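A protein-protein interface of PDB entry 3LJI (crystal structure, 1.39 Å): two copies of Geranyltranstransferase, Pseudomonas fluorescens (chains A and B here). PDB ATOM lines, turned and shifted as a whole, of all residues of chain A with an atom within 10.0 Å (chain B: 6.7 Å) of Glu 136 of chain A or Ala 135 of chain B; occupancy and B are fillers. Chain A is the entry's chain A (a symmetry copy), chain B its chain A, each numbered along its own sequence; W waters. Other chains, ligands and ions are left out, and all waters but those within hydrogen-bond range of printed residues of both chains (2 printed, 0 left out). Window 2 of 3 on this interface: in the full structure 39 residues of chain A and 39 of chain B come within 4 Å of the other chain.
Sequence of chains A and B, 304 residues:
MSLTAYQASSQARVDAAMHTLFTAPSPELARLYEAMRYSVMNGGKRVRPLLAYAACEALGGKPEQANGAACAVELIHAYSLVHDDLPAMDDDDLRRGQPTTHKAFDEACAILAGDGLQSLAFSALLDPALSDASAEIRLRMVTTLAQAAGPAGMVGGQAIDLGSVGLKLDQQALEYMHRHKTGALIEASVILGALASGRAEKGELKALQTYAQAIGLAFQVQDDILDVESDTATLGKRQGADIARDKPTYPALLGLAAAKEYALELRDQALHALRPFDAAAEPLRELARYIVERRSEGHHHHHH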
ATOM      1  N   LEU A 126       8.657  -0.406   3.312  1.00  0.00           N
ATOM      2  CA  LEU A 126       7.436  -0.472   4.104  1.00  0.00           C
ATOM      3  C   LEU A 126       6.969   0.901   4.618  1.00  0.00           C
ATOM      4  O   LEU A 126       6.019   0.988   5.411  1.00  0.00           O
ATOM      5  CB  LEU A 126       7.597  -1.493   5.230  1.00  0.00           C
ATOM      6  CG  LEU A 126       7.864  -2.930   4.765  1.00  0.00           C
ATOM      7  CD1 LEU A 126       7.889  -3.886   5.917  1.00  0.00           C
ATOM      8  CD2 LEU A 126       6.859  -3.392   3.712  1.00  0.00           C
ATOM      9  N   ASP A 132       1.675   2.353  -0.860  1.00  0.00           N
ATOM     10  CA  ASP A 132       0.368   2.005  -0.258  1.00  0.00           C
ATOM     11  C   ASP A 132      -0.222   0.612  -0.586  1.00  0.00           C
ATOM     12  O   ASP A 132      -1.433   0.427  -0.469  1.00  0.00           O
ATOM     13  CB  ASP A 132      -0.660   3.100  -0.607  1.00  0.00           C
ATOM     14  CG  ASP A 132      -1.922   3.040   0.266  1.00  0.00           C
ATOM     15  OD1 ASP A 132      -1.807   2.890   1.500  1.00  0.00           O
ATOM     16  OD2 ASP A 132      -3.036   3.140  -0.291  1.00  0.00           O
ATOM     17  N   ALA A 133       0.595  -0.373  -0.964  1.00  0.00           N
ATOM     18  CA  ALA A 133       0.062  -1.697  -1.377  1.00  0.00           C
ATOM     19  C   ALA A 133      -0.537  -2.491  -0.205  1.00  0.00           C
ATOM     20  O   ALA A 133      -0.298  -2.150   0.944  1.00  0.00           O
ATOM     21  CB  ALA A 133       1.143  -2.519  -2.076  1.00  0.00           C
ATOM     22  N   SER A 134      -1.316  -3.538  -0.497  1.00  0.00           N
ATOM     23  CA  SER A 134      -1.957  -4.356   0.548  1.00  0.00           C
ATOM     24  C   SER A 134      -0.955  -5.203   1.327  1.00  0.00           C
ATOM     25  O   SER A 134       0.191  -5.392   0.886  1.00  0.00           O
ATOM     26  CB  SER A 134      -3.053  -5.256  -0.056  1.00  0.00           C
ATOM     27  OG  SER A 134      -2.467  -6.357  -0.745  1.00  0.00           O
ATOM     28  N   ALA A 135      -1.361  -5.720   2.486  1.00  0.00           N
ATOM     29  CA  ALA A 135      -0.416  -6.419   3.374  1.00  0.00           C
ATOM     30  C   ALA A 135       0.117  -7.712   2.763  1.00  0.00           C
ATOM     31  O   ALA A 135       1.304  -7.969   2.831  1.00  0.00           O
ATOM     32  CB  ALA A 135      -1.029  -6.656   4.743  1.00  0.00           C
ATOM     33  N   GLU A 136      -0.729  -8.524   2.129  1.00  0.00           N
ATOM     34  CA  GLU A 136      -0.184  -9.733   1.498  1.00  0.00           C
ATOM     35  C   GLU A 136       0.765  -9.383   0.325  1.00  0.00           C
ATOM     36  O   GLU A 136       1.780 -10.061   0.131  1.00  0.00           O
ATOM     37  CB  GLU A 136      -1.279 -10.727   1.082  1.00  0.00           C
ATOM     38  CG  GLU A 136      -2.092 -11.312   2.257  1.00  0.00           C
ATOM     39  CD  GLU A 136      -1.257 -12.143   3.245  1.00  0.00           C
ATOM     40  OE1 GLU A 136      -0.287 -12.821   2.824  1.00  0.00           O
ATOM     41  OE2 GLU A 136      -1.587 -12.125   4.453  1.00  0.00           O
ATOM     42  N   ILE A 137       0.459  -8.321  -0.428  1.00  0.00           N
ATOM     43  CA  ILE A 137       1.349  -7.837  -1.502  1.00  0.00           C
ATOM     44  C   ILE A 137       2.681  -7.339  -0.934  1.00  0.00           C
ATOM     45  O   ILE A 137       3.759  -7.767  -1.401  1.00  0.00           O
ATOM     46  CB  ILE A 137       0.676  -6.752  -2.394  1.00  0.00           C
ATOM     47  CG1 ILE A 137      -0.478  -7.367  -3.205  1.00  0.00           C
ATOM     48  CG2 ILE A 137       1.700  -6.084  -3.323  1.00  0.00           C
ATOM     49  CD1 ILE A 137      -0.052  -8.223  -4.407  1.00  0.00           C
ATOM     50  N   ARG A 138       2.629  -6.449   0.056  1.00  0.00           N
ATOM     51  CA  ARG A 138       3.859  -5.988   0.718  1.00  0.00           C
ATOM     52  C   ARG A 138       4.706  -7.129   1.336  1.00  0.00           C
ATOM     53  O   ARG A 138       5.942  -7.061   1.328  1.00  0.00           O
ATOM     54  CB  ARG A 138       3.564  -4.954   1.782  1.00  0.00           C
ATOM     55  CG  ARG A 138       3.525  -3.518   1.312  1.00  0.00           C
ATOM     56  CD  ARG A 138       2.999  -2.646   2.431  1.00  0.00           C
ATOM     57  NE  ARG A 138       1.548  -2.814   2.563  1.00  0.00           N
ATOM     58  CZ  ARG A 138       0.883  -2.914   3.713  1.00  0.00           C
ATOM     59  NH1 ARG A 138       1.509  -2.890   4.882  1.00  0.00           N
ATOM     60  NH2 ARG A 138      -0.425  -3.068   3.692  1.00  0.00           N
ATOM     61  N   LEU A 139       4.059  -8.169   1.867  1.00  0.00           N
ATOM     62  CA  LEU A 139       4.771  -9.350   2.350  1.00  0.00           C
ATOM     63  C   LEU A 139       5.569  -9.986   1.216  1.00  0.00           C
ATOM     64  O   LEU A 139       6.718 -10.412   1.412  1.00  0.00           O
ATOM     65  CB  LEU A 139       3.807 -10.368   2.988  1.00  0.00           C
ATOM     66  CG  LEU A 139       4.394 -11.685   3.536  1.00  0.00           C
ATOM     67  CD1 LEU A 139       5.304 -11.491   4.735  1.00  0.00           C
ATOM     68  CD2 LEU A 139       3.277 -12.644   3.911  1.00  0.00           C
ATOM     69  N   ARG A 140       4.962 -10.091   0.039  1.00  0.00           N
ATOM     70  CA  ARG A 140       5.675 -10.600  -1.107  1.00  0.00           C
ATOM     71  C   ARG A 140       6.888  -9.697  -1.373  1.00  0.00           C
ATOM     72  O   ARG A 140       7.977 -10.214  -1.577  1.00  0.00           O
ATOM     73  CB  ARG A 140       4.768 -10.685  -2.333  1.00  0.00           C
ATOM     74  CG  ARG A 140       3.591 -11.652  -2.216  1.00  0.00           C
ATOM     75  CD  ARG A 140       2.388 -11.147  -3.028  1.00  0.00           C
ATOM     76  NE  ARG A 140       2.176 -11.741  -4.362  1.00  0.00           N
ATOM     77  CZ  ARG A 140       3.096 -12.291  -5.162  1.00  0.00           C
ATOM     78  NH1 ARG A 140       4.381 -12.361  -4.817  1.00  0.00           N
ATOM     79  NH2 ARG A 140       2.718 -12.778  -6.343  1.00  0.00           N
ATOM     80  N   MET A 141       6.717  -8.372  -1.264  1.00  0.00           N
ATOM     81  CA  MET A 141       7.780  -7.338  -1.478  1.00  0.00           C
ATOM     82  C   MET A 141       9.055  -7.553  -0.668  1.00  0.00           C
ATOM     83  O   MET A 141      10.172  -7.612  -1.200  1.00  0.00           O
ATOM     84  CB  MET A 141       7.275  -5.926  -1.098  1.00  0.00           C
ATOM     85  CG  MET A 141       6.759  -5.017  -2.210  1.00  0.00           C
ATOM     86  SD  MET A 141       6.633  -3.083  -1.730  1.00  0.00           S
ATOM     87  CE  MET A 141       5.516  -2.427  -3.177  1.00  0.00           C
ATOM     88  N   VAL A 142       8.911  -7.586   0.669  1.00  0.00           N
ATOM     89  CA  VAL A 142      10.069  -7.716   1.601  1.00  0.00           C
ATOM     90  C   VAL A 142      10.732  -9.080   1.468  1.00  0.00           C
ATOM     91  O   VAL A 142      11.964  -9.169   1.476  1.00  0.00           O
ATOM     92  CB  VAL A 142       9.743  -7.438   3.123  1.00  0.00           C
ATOM     93  CG1 VAL A 142      10.909  -7.827   4.043  1.00  0.00           C
ATOM     94  CG2 VAL A 142       9.414  -5.994   3.362  1.00  0.00           C
ATOM     95  N   THR A 143       9.915 -10.121   1.329  1.00  0.00           N
ATOM     96  CA  THR A 143      10.413 -11.490   1.135  1.00  0.00           C
ATOM     97  C   THR A 143      11.288 -11.523  -0.107  1.00  0.00           C
ATOM     98  O   THR A 143      12.403 -12.067  -0.089  1.00  0.00           O
ATOM     99  CB  THR A 143       9.246 -12.519   1.009  1.00  0.00           C
ATOM    100  OG1 THR A 143       8.364 -12.383   2.133  1.00  0.00           O
ATOM    101  CG2 THR A 143       9.791 -13.949   0.988  1.00  0.00           C
ATOM    102  N   THR A 144      10.797 -10.905  -1.169  1.00  0.00           N
ATOM    103  CA  THR A 144      11.469 -10.870  -2.448  1.00  0.00           C
ATOM    104  C   THR A 144      12.778 -10.111  -2.288  1.00  0.00           C
ATOM    105  O   THR A 144      13.813 -10.596  -2.755  1.00  0.00           O
ATOM    106  CB  THR A 144      10.575 -10.218  -3.513  1.00  0.00           C
ATOM    107  OG1 THR A 144       9.332 -10.940  -3.577  1.00  0.00           O
ATOM    108  CG2 THR A 144      11.229 -10.243  -4.875  1.00  0.00           C
ATOM    109  N   LEU A 195       4.519  -5.617  -8.367  1.00  0.00           N
ATOM    110  CA  LEU A 195       3.700  -5.841  -7.173  1.00  0.00           C
ATOM    111  C   LEU A 195       3.088  -4.538  -6.656  1.00  0.00           C
ATOM    112  O   LEU A 195       1.906  -4.521  -6.263  1.00  0.00           O
ATOM    113  CB  LEU A 195       4.520  -6.550  -6.085  1.00  0.00           C
ATOM    114  CG  LEU A 195       4.856  -8.033  -6.310  1.00  0.00           C
ATOM    115  CD1 LEU A 195       5.829  -8.505  -5.260  1.00  0.00           C
ATOM    116  CD2 LEU A 195       3.594  -8.891  -6.295  1.00  0.00           C
ATOM    117  N   ALA A 196       3.871  -3.456  -6.703  1.00  0.00           N
ATOM    118  CA  ALA A 196       3.486  -2.121  -6.220  1.00  0.00           C
ATOM    119  C   ALA A 196       2.241  -1.561  -6.877  1.00  0.00           C
ATOM    120  O   ALA A 196       1.564  -0.713  -6.278  1.00  0.00           O
ATOM    121  CB  ALA A 196       4.623  -1.138  -6.416  1.00  0.00           C
ATOM    122  N   GLY A 198      -0.357  -3.114  -7.329  1.00  0.00           N
ATOM    123  CA  GLY A 198      -1.500  -3.805  -6.690  1.00  0.00           C
ATOM    124  C   GLY A 198      -2.309  -4.695  -7.626  1.00  0.00           C
ATOM    125  O   GLY A 198      -3.288  -5.313  -7.204  1.00  0.00           O
ATOM    126  N   ALA A 200      -0.827  -7.051 -10.002  1.00  0.00           N
ATOM    127  CA  ALA A 200       0.039  -8.075 -10.602  1.00  0.00           C
ATOM    128  C   ALA A 200      -0.512  -9.501 -10.513  1.00  0.00           C
ATOM    129  O   ALA A 200      -0.645 -10.057  -9.422  1.00  0.00           O
ATOM    130  CB  ALA A 200       1.442  -8.007 -10.004  1.00  0.00           C
ATOM    131  N   LEU A 205       3.576 -11.596 -13.915  1.00  0.00           N
ATOM    132  CA  LEU A 205       4.801 -11.713 -13.129  1.00  0.00           C
ATOM    133  C   LEU A 205       5.790 -12.716 -13.723  1.00  0.00           C
ATOM    134  O   LEU A 205       7.000 -12.494 -13.656  1.00  0.00           O
ATOM    135  CB  LEU A 205       4.500 -12.079 -11.667  1.00  0.00           C
ATOM    136  CG  LEU A 205       3.834 -11.001 -10.802  1.00  0.00           C
ATOM    137  CD1 LEU A 205       3.199 -11.642  -9.572  1.00  0.00           C
ATOM    138  CD2 LEU A 205       4.813  -9.885 -10.394  1.00  0.00           C
ATOM    139  N   ALA B 133       2.218 -15.117  12.755  1.00  0.00           N
ATOM    140  CA  ALA B 133       1.424 -13.934  13.174  1.00  0.00           C
ATOM    141  C   ALA B 133       0.661 -13.284  12.008  1.00  0.00           C
ATOM    142  O   ALA B 133       0.956 -13.569  10.857  1.00  0.00           O
ATOM    143  CB  ALA B 133       2.314 -12.903  13.864  1.00  0.00           C
ATOM    144  N   SER B 134      -0.317 -12.424  12.308  1.00  0.00           N
ATOM    145  CA  SER B 134      -1.125 -11.759  11.270  1.00  0.00           C
ATOM    146  C   SER B 134      -0.329 -10.721  10.483  1.00  0.00           C
ATOM    147  O   SER B 134       0.756 -10.296  10.913  1.00  0.00           O
ATOM    148  CB  SER B 134      -2.380 -11.108  11.884  1.00  0.00           C
ATOM    149  OG  SER B 134      -2.031  -9.908  12.569  1.00  0.00           O
ATOM    150  N   ALA B 135      -0.845 -10.302   9.328  1.00  0.00           N
ATOM    151  CA  ALA B 135      -0.075  -9.421   8.432  1.00  0.00           C
ATOM    152  C   ALA B 135       0.180  -8.045   9.039  1.00  0.00           C
ATOM    153  O   ALA B 135       1.286  -7.545   8.961  1.00  0.00           O
ATOM    154  CB  ALA B 135      -0.737  -9.319   7.068  1.00  0.00           C
ATOM    155  N   GLU B 136      -0.812  -7.427   9.681  1.00  0.00           N
ATOM    156  CA  GLU B 136      -0.526  -6.130  10.309  1.00  0.00           C
ATOM    157  C   GLU B 136       0.486  -6.272  11.473  1.00  0.00           C
ATOM    158  O   GLU B 136       1.337  -5.397  11.659  1.00  0.00           O
ATOM    159  CB  GLU B 136      -1.801  -5.387  10.736  1.00  0.00           C
ATOM    160  CG  GLU B 136      -2.729  -4.987   9.568  1.00  0.00           C
ATOM    161  CD  GLU B 136      -2.096  -4.001   8.574  1.00  0.00           C
ATOM    162  OE1 GLU B 136      -1.286  -3.134   8.987  1.00  0.00           O
ATOM    163  OE2 GLU B 136      -2.425  -4.089   7.368  1.00  0.00           O
ATOM    164  N   ILE B 137       0.416  -7.375  12.228  1.00  0.00           N
ATOM    165  CA  ILE B 137       1.396  -7.661  13.294  1.00  0.00           C
ATOM    166  C   ILE B 137       2.798  -7.869  12.713  1.00  0.00           C
ATOM    167  O   ILE B 137       3.767  -7.224  13.171  1.00  0.00           O
ATOM    168  CB  ILE B 137       0.973  -8.861  14.191  1.00  0.00           C
ATOM    169  CG1 ILE B 137      -0.276  -8.501  15.012  1.00  0.00           C
ATOM    170  CG2 ILE B 137       2.123  -9.299  15.110  1.00  0.00           C
ATOM    171  CD1 ILE B 137      -0.028  -7.574  16.211  1.00  0.00           C
ATOM    172  N   ARG B 138       2.926  -8.751  11.722  1.00  0.00           N
ATOM    173  CA  ARG B 138       4.218  -8.945  11.049  1.00  0.00           C
ATOM    174  C   ARG B 138       4.803  -7.652  10.425  1.00  0.00           C
ATOM    175  O   ARG B 138       6.025  -7.459  10.422  1.00  0.00           O
ATOM    176  CB  ARG B 138       4.137 -10.018   9.988  1.00  0.00           C
ATOM    177  CG  ARG B 138       4.405 -11.430  10.457  1.00  0.00           C
ATOM    178  CD  ARG B 138       4.063 -12.395   9.341  1.00  0.00           C
ATOM    179  NE  ARG B 138       2.607 -12.535   9.222  1.00  0.00           N
ATOM    180  CZ  ARG B 138       1.926 -12.576   8.078  1.00  0.00           C
ATOM    181  NH1 ARG B 138       2.533 -12.470   6.903  1.00  0.00           N
ATOM    182  NH2 ARG B 138       0.616 -12.700   8.111  1.00  0.00           N
ATOM    183  N   LEU B 139       3.947  -6.772   9.900  1.00  0.00           N
ATOM    184  CA  LEU B 139       4.392  -5.468   9.413  1.00  0.00           C
ATOM    185  C   LEU B 139       5.048  -4.677  10.540  1.00  0.00           C
ATOM    186  O   LEU B 139       6.081  -4.020  10.334  1.00  0.00           O
ATOM    187  CB  LEU B 139       3.230  -4.675   8.784  1.00  0.00           C
ATOM    188  CG  LEU B 139       3.523  -3.265   8.232  1.00  0.00           C
ATOM    189  CD1 LEU B 139       4.443  -3.264   7.025  1.00  0.00           C
ATOM    190  CD2 LEU B 139       2.227  -2.561   7.868  1.00  0.00           C
ATOM    191  N   ARG B 140       4.444  -4.701  11.722  1.00  0.00           N
ATOM    192  CA  ARG B 140       5.044  -4.053  12.862  1.00  0.00           C
ATOM    193  C   ARG B 140       6.422  -4.681  13.117  1.00  0.00           C
ATOM    194  O   ARG B 140       7.380  -3.948  13.312  1.00  0.00           O
ATOM    195  CB  ARG B 140       4.150  -4.158  14.097  1.00  0.00           C
ATOM    196  CG  ARG B 140       2.796  -3.460  13.991  1.00  0.00           C
ATOM    197  CD  ARG B 140       1.733  -4.204  14.813  1.00  0.00           C
ATOM    198  NE  ARG B 140       1.412  -3.668  16.150  1.00  0.00           N
ATOM    199  CZ  ARG B 140       2.204  -2.936  16.942  1.00  0.00           C
ATOM    200  NH1 ARG B 140       3.443  -2.599  16.586  1.00  0.00           N
ATOM    201  NH2 ARG B 140       1.743  -2.538  18.126  1.00  0.00           N
HETATM  202  O   HOH W   1      -1.458 -13.345   6.903  1.00  0.00           O
HETATM  203  O   HOH W   2      -2.577  -2.871   4.919  1.00  0.00           O
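The backbone carbonyl oxygen of Ala 133 of chain B is in hydrogen-bond range of the guanidinium group of Arg 138 of chain B, 2.5 Å away.
The backbone carbonyl oxygen (O) of Ser 134 of chain B is in hydrogen-bond range of the guanidinium group (NE) of Arg 138 of chain B (3.4 Å).
NE of Arg 138 of chain A sits at hydrogen-bond distance from O of Ala 133 of chain A (2.5 Å).
The guanidinium group (NE) of Arg 138 of chain A is in hydrogen-bond range of the backbone carbonyl oxygen (O) of Ser 134 of chain A (3.4 Å).
OG1 of Thr 143 of chain A is in hydrogen-bond range of O of Leu 139 of chain A (2.7 Å).
Among the printed residues, merely in contact across the chains: Leu 139 of chain A with Arg 138 of chain B, Arg 138 of chain A with Leu 139 of chain B, Ala 135 of chain A with Ala 135 of chain B, Leu 126 of chain A with Leu 139 of chain B, Ala 135 of chain A with Glu 136 of chain B and Glu 136 of chain A with Ala 135 of chain B.
Of chain A, only Ala 135 (3.5 Å) and Glu 136 (3.9 Å) come within 4 Å of Ala 135 of chain B.
Ser 134 of chain B touches none of the printed residues of chain A.
Glu 136 of chain B touches just one residue of chain A: Ala 135.
Arg 138 of chain B touches one residue of chain A.
Of the printed residues of chain B, Leu 126 of chain A touches Leu 139.
Of the printed residues of chain B, Ala 135 of chain A touches Ala 135 (3.5 Å) and Glu 136 (3.9 Å).
Of the printed residues of chain B, Arg 138 of chain A touches Leu 139.
Printed residues of chain B within 4 Å of Leu 139 of chain A: Arg 138.
The nearest residue of chain B that does not touch Glu 136 of chain A is Arg 138 of chain B (4.3 Å).
The nearest residue of chain A that does not touch Ala 135 of chain B is Leu 139 of chain A (6.1 Å).
The nearest printed residue of chain B that does not touch Leu 139 of chain A is Ala 135 of chain B (6.1 Å).
Along chain B the printed residues that touch a printed residue of chain A span positions 135 to 139.
Hydrophobic or aromatic side chains of chain A that line the printed part of chain B: Leu 126, Ala 135 and Leu 139.
Among the printed residues, no Asp or Glu carboxylate lies within 4 Å of a Lys or Arg side-chain nitrogen of the other chain.
Ala 135 of chain B touches its own counterpart, Ala 135 of chain A.
Ala 135 of chain A touches Glu 136 of chain B, and with the chains exchanged Glu 136 of chain A touches Ala 135 of chain B.
Arg 138 of chain A touches Leu 139 of chain B, and with the chains exchanged Leu 139 of chain A touches Arg 138 of chain B.
8 positions are printed for both chains.
Water W1 bridges NH2 of Arg 138 of chain B (2.5 Å) and OE2 of Glu 136 of chain A (2.7 Å).
Water W2 bridges NH2 of Arg 138 of chain A (2.5 Å) and OE2 of Glu 136 of chain B (2.7 Å).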
